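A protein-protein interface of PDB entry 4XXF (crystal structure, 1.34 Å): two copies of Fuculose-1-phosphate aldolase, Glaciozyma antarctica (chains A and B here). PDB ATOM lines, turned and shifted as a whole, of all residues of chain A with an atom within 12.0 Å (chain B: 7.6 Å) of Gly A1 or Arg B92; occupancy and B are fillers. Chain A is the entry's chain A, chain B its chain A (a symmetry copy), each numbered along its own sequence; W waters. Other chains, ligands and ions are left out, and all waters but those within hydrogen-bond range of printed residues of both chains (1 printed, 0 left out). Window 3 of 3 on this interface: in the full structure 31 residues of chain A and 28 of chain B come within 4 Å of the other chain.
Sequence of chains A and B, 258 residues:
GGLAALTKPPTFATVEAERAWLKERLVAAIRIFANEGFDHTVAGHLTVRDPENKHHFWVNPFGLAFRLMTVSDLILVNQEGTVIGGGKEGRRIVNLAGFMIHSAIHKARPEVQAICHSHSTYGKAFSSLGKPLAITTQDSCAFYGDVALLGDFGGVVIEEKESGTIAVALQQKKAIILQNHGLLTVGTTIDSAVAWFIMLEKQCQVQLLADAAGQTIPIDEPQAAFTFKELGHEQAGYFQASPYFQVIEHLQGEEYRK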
ATOM      1  N   GLY A   1      -7.636  14.943   5.321  1.00  0.00           N
ATOM      2  CA  GLY A   1      -6.875  13.877   5.953  1.00  0.00           C
ATOM      3  C   GLY A   1      -6.988  12.549   5.224  1.00  0.00           C
ATOM      4  O   GLY A   1      -7.487  12.497   4.097  1.00  0.00           O
ATOM      5  N   GLY A   2      -6.511  11.474   5.853  1.00  0.00           N
ATOM      6  CA  GLY A   2      -5.837  11.555   7.139  1.00  0.00           C
ATOM      7  C   GLY A   2      -6.658  11.093   8.333  1.00  0.00           C
ATOM      8  O   GLY A   2      -6.624  11.719   9.393  1.00  0.00           O
ATOM      9  N   LEU A   3      -7.385   9.992   8.175  1.00  0.00           N
ATOM     10  CA  LEU A   3      -8.246   9.495   9.248  1.00  0.00           C
ATOM     11  C   LEU A   3      -7.451   8.907  10.415  1.00  0.00           C
ATOM     12  O   LEU A   3      -7.834   9.073  11.572  1.00  0.00           O
ATOM     13  CB  LEU A   3      -9.220   8.449   8.706  1.00  0.00           C
ATOM     14  CG  LEU A   3     -10.158   7.800   9.725  1.00  0.00           C
ATOM     15  CD1 LEU A   3     -11.017   8.849  10.425  1.00  0.00           C
ATOM     16  CD2 LEU A   3     -11.031   6.767   9.041  1.00  0.00           C
ATOM     17  N   ALA A   4      -6.348   8.227  10.112  1.00  0.00           N
ATOM     18  CA  ALA A   4      -5.544   7.567  11.140  1.00  0.00           C
ATOM     19  C   ALA A   4      -5.104   8.523  12.253  1.00  0.00           C
ATOM     20  O   ALA A   4      -5.186   8.181  13.432  1.00  0.00           O
ATOM     21  CB  ALA A   4      -4.330   6.904  10.509  1.00  0.00           C
ATOM     22  N   ALA A   5      -4.658   9.721  11.878  1.00  0.00           N
ATOM     23  CA  ALA A   5      -4.203  10.723  12.846  1.00  0.00           C
ATOM     24  C   ALA A   5      -5.323  11.176  13.776  1.00  0.00           C
ATOM     25  O   ALA A   5      -5.072  11.659  14.881  1.00  0.00           O
ATOM     26  CB  ALA A   5      -3.615  11.926  12.121  1.00  0.00           C
ATOM     27  N   LEU A   6      -6.560  11.023  13.321  1.00  0.00           N
ATOM     28  CA  LEU A   6      -7.712  11.461  14.096  1.00  0.00           C
ATOM     29  C   LEU A   6      -8.183  10.399  15.085  1.00  0.00           C
ATOM     30  O   LEU A   6      -9.057  10.662  15.903  1.00  0.00           O
ATOM     31  CB  LEU A   6      -8.860  11.844  13.160  1.00  0.00           C
ATOM     32  CG  LEU A   6      -8.590  13.017  12.216  1.00  0.00           C
ATOM     33  CD1 LEU A   6      -9.721  13.153  11.218  1.00  0.00           C
ATOM     34  CD2 LEU A   6      -8.407  14.307  12.997  1.00  0.00           C
ATOM     35  N   THR A   7      -7.600   9.205  15.016  1.00  0.00           N
ATOM     36  CA  THR A   7      -8.051   8.090  15.842  1.00  0.00           C
ATOM     37  C   THR A   7      -7.061   7.778  16.949  1.00  0.00           C
ATOM     38  O   THR A   7      -7.204   6.788  17.664  1.00  0.00           O
ATOM     39  CB  THR A   7      -8.262   6.815  15.014  1.00  0.00           C
ATOM     40  OG1 THR A   7      -6.997   6.340  14.533  1.00  0.00           O
ATOM     41  CG2 THR A   7      -9.182   7.080  13.834  1.00  0.00           C
ATOM     42  N   PHE A 239     -12.049   7.862  18.123  1.00  0.00           N
ATOM     43  CA  PHE A 239     -12.702   8.682  17.108  1.00  0.00           C
ATOM     44  C   PHE A 239     -14.165   8.979  17.470  1.00  0.00           C
ATOM     45  O   PHE A 239     -14.657  10.104  17.286  1.00  0.00           O
ATOM     46  CB  PHE A 239     -12.609   7.980  15.749  1.00  0.00           C
ATOM     47  CG  PHE A 239     -12.967   8.852  14.583  1.00  0.00           C
ATOM     48  CD1 PHE A 239     -12.187   9.949  14.255  1.00  0.00           C
ATOM     49  CD2 PHE A 239     -14.059   8.554  13.787  1.00  0.00           C
ATOM     50  CE1 PHE A 239     -12.510  10.750  13.167  1.00  0.00           C
ATOM     51  CE2 PHE A 239     -14.384   9.352  12.697  1.00  0.00           C
ATOM     52  CZ  PHE A 239     -13.601  10.445  12.391  1.00  0.00           C
ATOM     53  N   GLN A 246     -14.563  18.082  21.076  1.00  0.00           N
ATOM     54  CA  GLN A 246     -14.585  19.320  20.304  1.00  0.00           C
ATOM     55  C   GLN A 246     -15.591  20.300  20.889  1.00  0.00           C
ATOM     56  O   GLN A 246     -15.287  21.473  21.092  1.00  0.00           O
ATOM     57  CB  GLN A 246     -14.946  19.058  18.848  1.00  0.00           C
ATOM     58  CG  GLN A 246     -13.962  18.223  18.052  1.00  0.00           C
ATOM     59  CD  GLN A 246     -14.644  17.574  16.862  1.00  0.00           C
ATOM     60  OE1 GLN A 246     -15.625  18.099  16.332  1.00  0.00           O
ATOM     61  NE2 GLN A 246     -14.135  16.428  16.430  1.00  0.00           N
ATOM     62  N   PRO B  61     -18.051  16.461   6.904  1.00  0.00           N
ATOM     63  CA  PRO B  61     -16.805  15.692   6.960  1.00  0.00           C
ATOM     64  C   PRO B  61     -16.784  14.774   8.178  1.00  0.00           C
ATOM     65  O   PRO B  61     -17.293  15.140   9.239  1.00  0.00           O
ATOM     66  CB  PRO B  61     -15.731  16.774   7.053  1.00  0.00           C
ATOM     67  CG  PRO B  61     -16.419  17.896   7.787  1.00  0.00           C
ATOM     68  CD  PRO B  61     -17.847  17.875   7.283  1.00  0.00           C
ATOM     69  N   PHE B  62     -16.209  13.596   8.022  1.00  0.00           N
ATOM     70  CA  PHE B  62     -16.255  12.558   9.045  1.00  0.00           C
ATOM     71  C   PHE B  62     -15.613  13.008  10.354  1.00  0.00           C
ATOM     72  O   PHE B  62     -14.471  13.449  10.374  1.00  0.00           O
ATOM     73  CB  PHE B  62     -15.553  11.306   8.498  1.00  0.00           C
ATOM     74  CG  PHE B  62     -15.919  10.006   9.186  1.00  0.00           C
ATOM     75  CD1 PHE B  62     -17.059   9.868   9.968  1.00  0.00           C
ATOM     76  CD2 PHE B  62     -15.099   8.899   9.012  1.00  0.00           C
ATOM     77  CE1 PHE B  62     -17.360   8.647  10.566  1.00  0.00           C
ATOM     78  CE2 PHE B  62     -15.398   7.688   9.604  1.00  0.00           C
ATOM     79  CZ  PHE B  62     -16.528   7.566  10.388  1.00  0.00           C
ATOM     80  N   SER B  72     -17.438  26.271   5.650  1.00  0.00           N
ATOM     81  CA  SER B  72     -16.069  25.953   5.236  1.00  0.00           C
ATOM     82  C   SER B  72     -15.675  24.500   5.481  1.00  0.00           C
ATOM     83  O   SER B  72     -14.709  24.007   4.897  1.00  0.00           O
ATOM     84  CB  SER B  72     -15.080  26.869   5.958  1.00  0.00           C
ATOM     85  OG  SER B  72     -15.198  28.198   5.481  1.00  0.00           O
ATOM     86  N   ASP B  73     -16.414  23.809   6.347  1.00  0.00           N
ATOM     87  CA  ASP B  73     -16.104  22.416   6.653  1.00  0.00           C
ATOM     88  C   ASP B  73     -16.644  21.422   5.639  1.00  0.00           C
ATOM     89  O   ASP B  73     -16.129  20.305   5.528  1.00  0.00           O
ATOM     90  CB  ASP B  73     -16.673  22.042   8.021  1.00  0.00           C
ATOM     91  CG  ASP B  73     -16.022  22.800   9.149  1.00  0.00           C
ATOM     92  OD1 ASP B  73     -14.784  22.708   9.293  1.00  0.00           O
ATOM     93  OD2 ASP B  73     -16.754  23.486   9.899  1.00  0.00           O
ATOM     94  N   LEU B  74     -17.707  21.796   4.926  1.00  0.00           N
ATOM     95  CA  LEU B  74     -18.352  20.857   4.013  1.00  0.00           C
ATOM     96  C   LEU B  74     -17.407  20.395   2.921  1.00  0.00           C
ATOM     97  O   LEU B  74     -16.635  21.192   2.374  1.00  0.00           O
ATOM     98  CB  LEU B  74     -19.573  21.478   3.350  1.00  0.00           C
ATOM     99  CG  LEU B  74     -20.715  21.901   4.261  1.00  0.00           C
ATOM    100  CD1 LEU B  74     -21.862  22.357   3.373  1.00  0.00           C
ATOM    101  CD2 LEU B  74     -21.147  20.751   5.193  1.00  0.00           C
ATOM    102  N   ILE B  75     -17.509  19.120   2.561  1.00  0.00           N
ATOM    103  CA  ILE B  75     -16.683  18.563   1.499  1.00  0.00           C
ATOM    104  C   ILE B  75     -17.536  18.147   0.315  1.00  0.00           C
ATOM    105  O   ILE B  75     -18.727  17.860   0.460  1.00  0.00           O
ATOM    106  CB  ILE B  75     -15.860  17.350   1.987  1.00  0.00           C
ATOM    107  CG1 ILE B  75     -16.742  16.341   2.728  1.00  0.00           C
ATOM    108  CG2 ILE B  75     -14.697  17.813   2.871  1.00  0.00           C
ATOM    109  CD1 ILE B  75     -16.075  14.995   2.969  1.00  0.00           C
ATOM    110  N   THR B  82     -15.105   9.503  -3.876  1.00  0.00           N
ATOM    111  CA  THR B  82     -13.856  10.265  -3.874  1.00  0.00           C
ATOM    112  C   THR B  82     -14.105  11.699  -3.397  1.00  0.00           C
ATOM    113  O   THR B  82     -14.991  12.379  -3.905  1.00  0.00           O
ATOM    114  CB  THR B  82     -13.206  10.285  -5.271  1.00  0.00           C
ATOM    115  OG1 THR B  82     -13.087   8.943  -5.750  1.00  0.00           O
ATOM    116  CG2 THR B  82     -11.821  10.920  -5.211  1.00  0.00           C
ATOM    117  N   VAL B  83     -13.341  12.147  -2.405  1.00  0.00           N
ATOM    118  CA  VAL B  83     -13.406  13.531  -1.957  1.00  0.00           C
ATOM    119  C   VAL B  83     -12.691  14.398  -2.979  1.00  0.00           C
ATOM    120  O   VAL B  83     -11.494  14.228  -3.213  1.00  0.00           O
ATOM    121  CB  VAL B  83     -12.774  13.714  -0.560  1.00  0.00           C
ATOM    122  CG1 VAL B  83     -12.831  15.168  -0.132  1.00  0.00           C
ATOM    123  CG2 VAL B  83     -13.470  12.828   0.459  1.00  0.00           C
ATOM    124  N   ILE B  84     -13.417  15.314  -3.606  1.00  0.00           N
ATOM    125  CA  ILE B  84     -12.860  16.059  -4.734  1.00  0.00           C
ATOM    126  C   ILE B  84     -12.830  17.568  -4.518  1.00  0.00           C
ATOM    127  O   ILE B  84     -12.368  18.307  -5.376  1.00  0.00           O
ATOM    128  CB  ILE B  84     -13.634  15.764  -6.039  1.00  0.00           C
ATOM    129  CG1 ILE B  84     -15.121  16.099  -5.878  1.00  0.00           C
ATOM    130  CG2 ILE B  84     -13.442  14.309  -6.461  1.00  0.00           C
ATOM    131  CD1 ILE B  84     -15.876  16.138  -7.197  1.00  0.00           C
ATOM    132  N   GLY B  85     -13.314  18.036  -3.376  1.00  0.00           N
ATOM    133  CA  GLY B  85     -13.248  19.457  -3.100  1.00  0.00           C
ATOM    134  C   GLY B  85     -13.708  19.840  -1.711  1.00  0.00           C
ATOM    135  O   GLY B  85     -14.240  19.013  -0.976  1.00  0.00           O
ATOM    136  N   GLY B  86     -13.493  21.103  -1.355  1.00  0.00           N
ATOM    137  CA  GLY B  86     -13.985  21.643  -0.102  1.00  0.00           C
ATOM    138  C   GLY B  86     -13.220  21.215   1.130  1.00  0.00           C
ATOM    139  O   GLY B  86     -12.127  20.647   1.053  1.00  0.00           O
ATOM    140  N   GLY B  87     -13.801  21.511   2.285  1.00  0.00           N
ATOM    141  CA  GLY B  87     -13.237  21.088   3.550  1.00  0.00           C
ATOM    142  C   GLY B  87     -12.020  21.850   4.032  1.00  0.00           C
ATOM    143  O   GLY B  87     -11.521  22.765   3.377  1.00  0.00           O
ATOM    144  N   LYS B  88     -11.547  21.435   5.199  1.00  0.00           N
ATOM    145  CA  LYS B  88     -10.346  21.978   5.802  1.00  0.00           C
ATOM    146  C   LYS B  88      -9.251  20.924   5.831  1.00  0.00           C
ATOM    147  O   LYS B  88      -9.530  19.728   5.944  1.00  0.00           O
ATOM    148  CB  LYS B  88     -10.634  22.474   7.217  1.00  0.00           C
ATOM    149  CG  LYS B  88     -11.583  23.667   7.270  1.00  0.00           C
ATOM    150  CD  LYS B  88     -11.835  24.082   8.703  1.00  0.00           C
ATOM    151  CE  LYS B  88     -12.870  25.183   8.789  1.00  0.00           C
ATOM    152  NZ  LYS B  88     -13.267  25.425  10.206  1.00  0.00           N
ATOM    153  N   GLU B  89      -8.013  21.389   5.709  1.00  0.00           N
ATOM    154  CA  GLU B  89      -6.817  20.573   5.889  1.00  0.00           C
ATOM    155  C   GLU B  89      -6.945  19.704   7.132  1.00  0.00           C
ATOM    156  O   GLU B  89      -7.207  20.215   8.222  1.00  0.00           O
ATOM    157  CB  GLU B  89      -5.588  21.478   6.014  1.00  0.00           C
ATOM    158  CG  GLU B  89      -4.213  20.796   5.942  1.00  0.00           C
ATOM    159  CD  GLU B  89      -4.011  19.945   4.696  1.00  0.00           C
ATOM    160  OE1 GLU B  89      -4.677  20.207   3.668  1.00  0.00           O
ATOM    161  OE2 GLU B  89      -3.165  19.023   4.739  1.00  0.00           O
ATOM    162  N   GLY B  90      -6.773  18.396   6.975  1.00  0.00           N
ATOM    163  CA  GLY B  90      -6.821  17.498   8.117  1.00  0.00           C
ATOM    164  C   GLY B  90      -8.143  16.763   8.271  1.00  0.00           C
ATOM    165  O   GLY B  90      -8.213  15.770   8.994  1.00  0.00           O
ATOM    166  N   ARG B  91      -9.197  17.226   7.603  1.00  0.00           N
ATOM    167  CA  ARG B  91     -10.477  16.517   7.669  1.00  0.00           C
ATOM    168  C   ARG B  91     -11.210  16.573   6.336  1.00  0.00           C
ATOM    169  O   ARG B  91     -12.401  16.858   6.262  1.00  0.00           O
ATOM    170  CB  ARG B  91     -11.365  17.073   8.793  1.00  0.00           C
ATOM    171  CG  ARG B  91     -12.404  16.064   9.289  1.00  0.00           C
ATOM    172  CD  ARG B  91     -13.434  16.661  10.244  1.00  0.00           C
ATOM    173  NE  ARG B  91     -12.844  17.065  11.520  1.00  0.00           N
ATOM    174  CZ  ARG B  91     -12.585  16.228  12.524  1.00  0.00           C
ATOM    175  NH1 ARG B  91     -12.876  14.941  12.406  1.00  0.00           N
ATOM    176  NH2 ARG B  91     -12.041  16.681  13.643  1.00  0.00           N
ATOM    177  N   ARG B  92     -10.477  16.299   5.268  1.00  0.00           N
ATOM    178  CA  ARG B  92     -11.092  16.117   3.963  1.00  0.00           C
ATOM    179  C   ARG B  92     -11.359  14.633   3.782  1.00  0.00           C
ATOM    180  O   ARG B  92     -10.768  13.963   2.933  1.00  0.00           O
ATOM    181  CB  ARG B  92     -10.200  16.697   2.868  1.00  0.00           C
ATOM    182  CG  ARG B  92     -10.216  18.214   2.919  1.00  0.00           C
ATOM    183  CD  ARG B  92      -9.159  18.877   2.069  1.00  0.00           C
ATOM    184  NE  ARG B  92      -9.348  20.322   2.144  1.00  0.00           N
ATOM    185  CZ  ARG B  92      -8.373  21.219   2.112  1.00  0.00           C
ATOM    186  NH1 ARG B  92      -7.110  20.833   1.991  1.00  0.00           N
ATOM    187  NH2 ARG B  92      -8.668  22.510   2.196  1.00  0.00           N
ATOM    188  N   ILE B  93     -12.271  14.145   4.620  1.00  0.00           N
ATOM    189  CA  ILE B  93     -12.585  12.726   4.697  1.00  0.00           C
ATOM    190  C   ILE B  93     -14.080  12.511   4.830  1.00  0.00           C
ATOM    191  O   ILE B  93     -14.779  13.273   5.495  1.00  0.00           O
ATOM    192  CB  ILE B  93     -11.870  12.037   5.886  1.00  0.00           C
ATOM    193  CG1 ILE B  93     -12.139  12.789   7.193  1.00  0.00           C
ATOM    194  CG2 ILE B  93     -10.380  11.931   5.626  1.00  0.00           C
ATOM    195  CD1 ILE B  93     -11.691  12.027   8.429  1.00  0.00           C
ATOM    196  N   VAL B  94     -14.572  11.467   4.176  1.00  0.00           N
ATOM    197  CA  VAL B  94     -15.979  11.111   4.227  1.00  0.00           C
ATOM    198  C   VAL B  94     -16.120   9.738   4.877  1.00  0.00           C
ATOM    199  O   VAL B  94     -15.254   8.877   4.726  1.00  0.00           O
ATOM    200  CB  VAL B  94     -16.624  11.119   2.807  1.00  0.00           C
ATOM    201  CG1 VAL B  94     -16.085   9.974   1.940  1.00  0.00           C
ATOM    202  CG2 VAL B  94     -18.143  11.062   2.894  1.00  0.00           C
HETATM  203  O   HOH W   1     -12.248  13.886  15.014  1.00  0.00           O
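The side-chain amide nitrogen (NE2) of Gln A246 sits close to the guanidinium group (NH2) of Arg B91, at 3.5 Å. The backbone NH (N) of Arg B92 sits close to the backbone NH (N) of Gly A1, 3.1 Å away.
The backbone carbonyl oxygen of Phe B62 lies within hydrogen-bond range of the guanidinium group of Arg B91, at 3.0 Å. OE1 of Glu B89 is in salt-bridge range of NH1 of Arg B92, at 3.0 Å. NE of Arg B92 sits at hydrogen-bond distance from O of Gly B86. O of Gly B87 lies within hydrogen-bond range of NH2 of Arg B92 (3.1 Å). N of Phe B62 lies within hydrogen-bond range of O of Ile B93, 2.9 Å away.
Gly A1 touches Gly B90. Arg B91 touches Gly A1 (N to N, 3.6 Å). O of Gly A1 touches CG2 of Ile B93, 3.3 Å away. Ile B93 touches Gly A2. CD1 of Leu A3 touches CD1 of Ile B93 (3.8 Å). Leu A6 touches Gly B90 (CD1 to O, 3.8 Å). Leu A6 touches Arg B91 (CD1 to NH1, 3.8 Å). CD1 of Ile B93 touches CD1 of Leu A6, 3.6 Å away. Phe A239 touches Phe B62.
Of the printed residues of chain B, Gly A1 touches Gly B90, Arg B91, Arg B92 and Ile B93. Printed residues of chain B within 4 Å of Leu A6: Gly B90 (3.8 Å), Arg B91 (3.8 Å) and Ile B93 (3.6 Å). Printed residues of chain B within 4 Å of Phe A239: Phe B62. Printed residues of chain B within 4 Å of Gln A246: Arg B91. No residue of chain A comes within 4 Å of Gly B86. No residue of chain A comes within 4 Å of Gly B87. Glu B89 touches none of the printed residues of chain A. Printed residues of chain A within 4 Å of Arg B91: Gly A1, Leu A6 and Gln A246. Arg B92 touches just one residue of chain A: Gly A1. No residue of chain A comes within 4 Å of Val B94. The nearest printed residue of chain B that does not touch Gly A1 is Glu B89 (5.1 Å). The nearest residue of chain A that does not touch Arg B92 is Gly A2 (5.7 Å). The nearest printed residue of chain B that does not touch Leu A6 is Phe B62 (4.8 Å).
Of the 9 printed residues of chain A, 6 touch a printed residue of chain B. Hydrophobic or aromatic side chains of chain A that line the printed part of chain B: Leu A3, Leu A6 and Phe A239. Along chain A the printed residues that touch a printed residue of chain B span positions 1 to 246. Among the printed residues, 11 pairs touch across the chains.
No position is printed for both chains. Of the 11 pairs that touch across the chains among the printed residues, none has its exchanged pair printed and touching as well.
Water W1 lies within hydrogen-bond range of NH1 of Arg B91 and NE2 of Gln A246.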
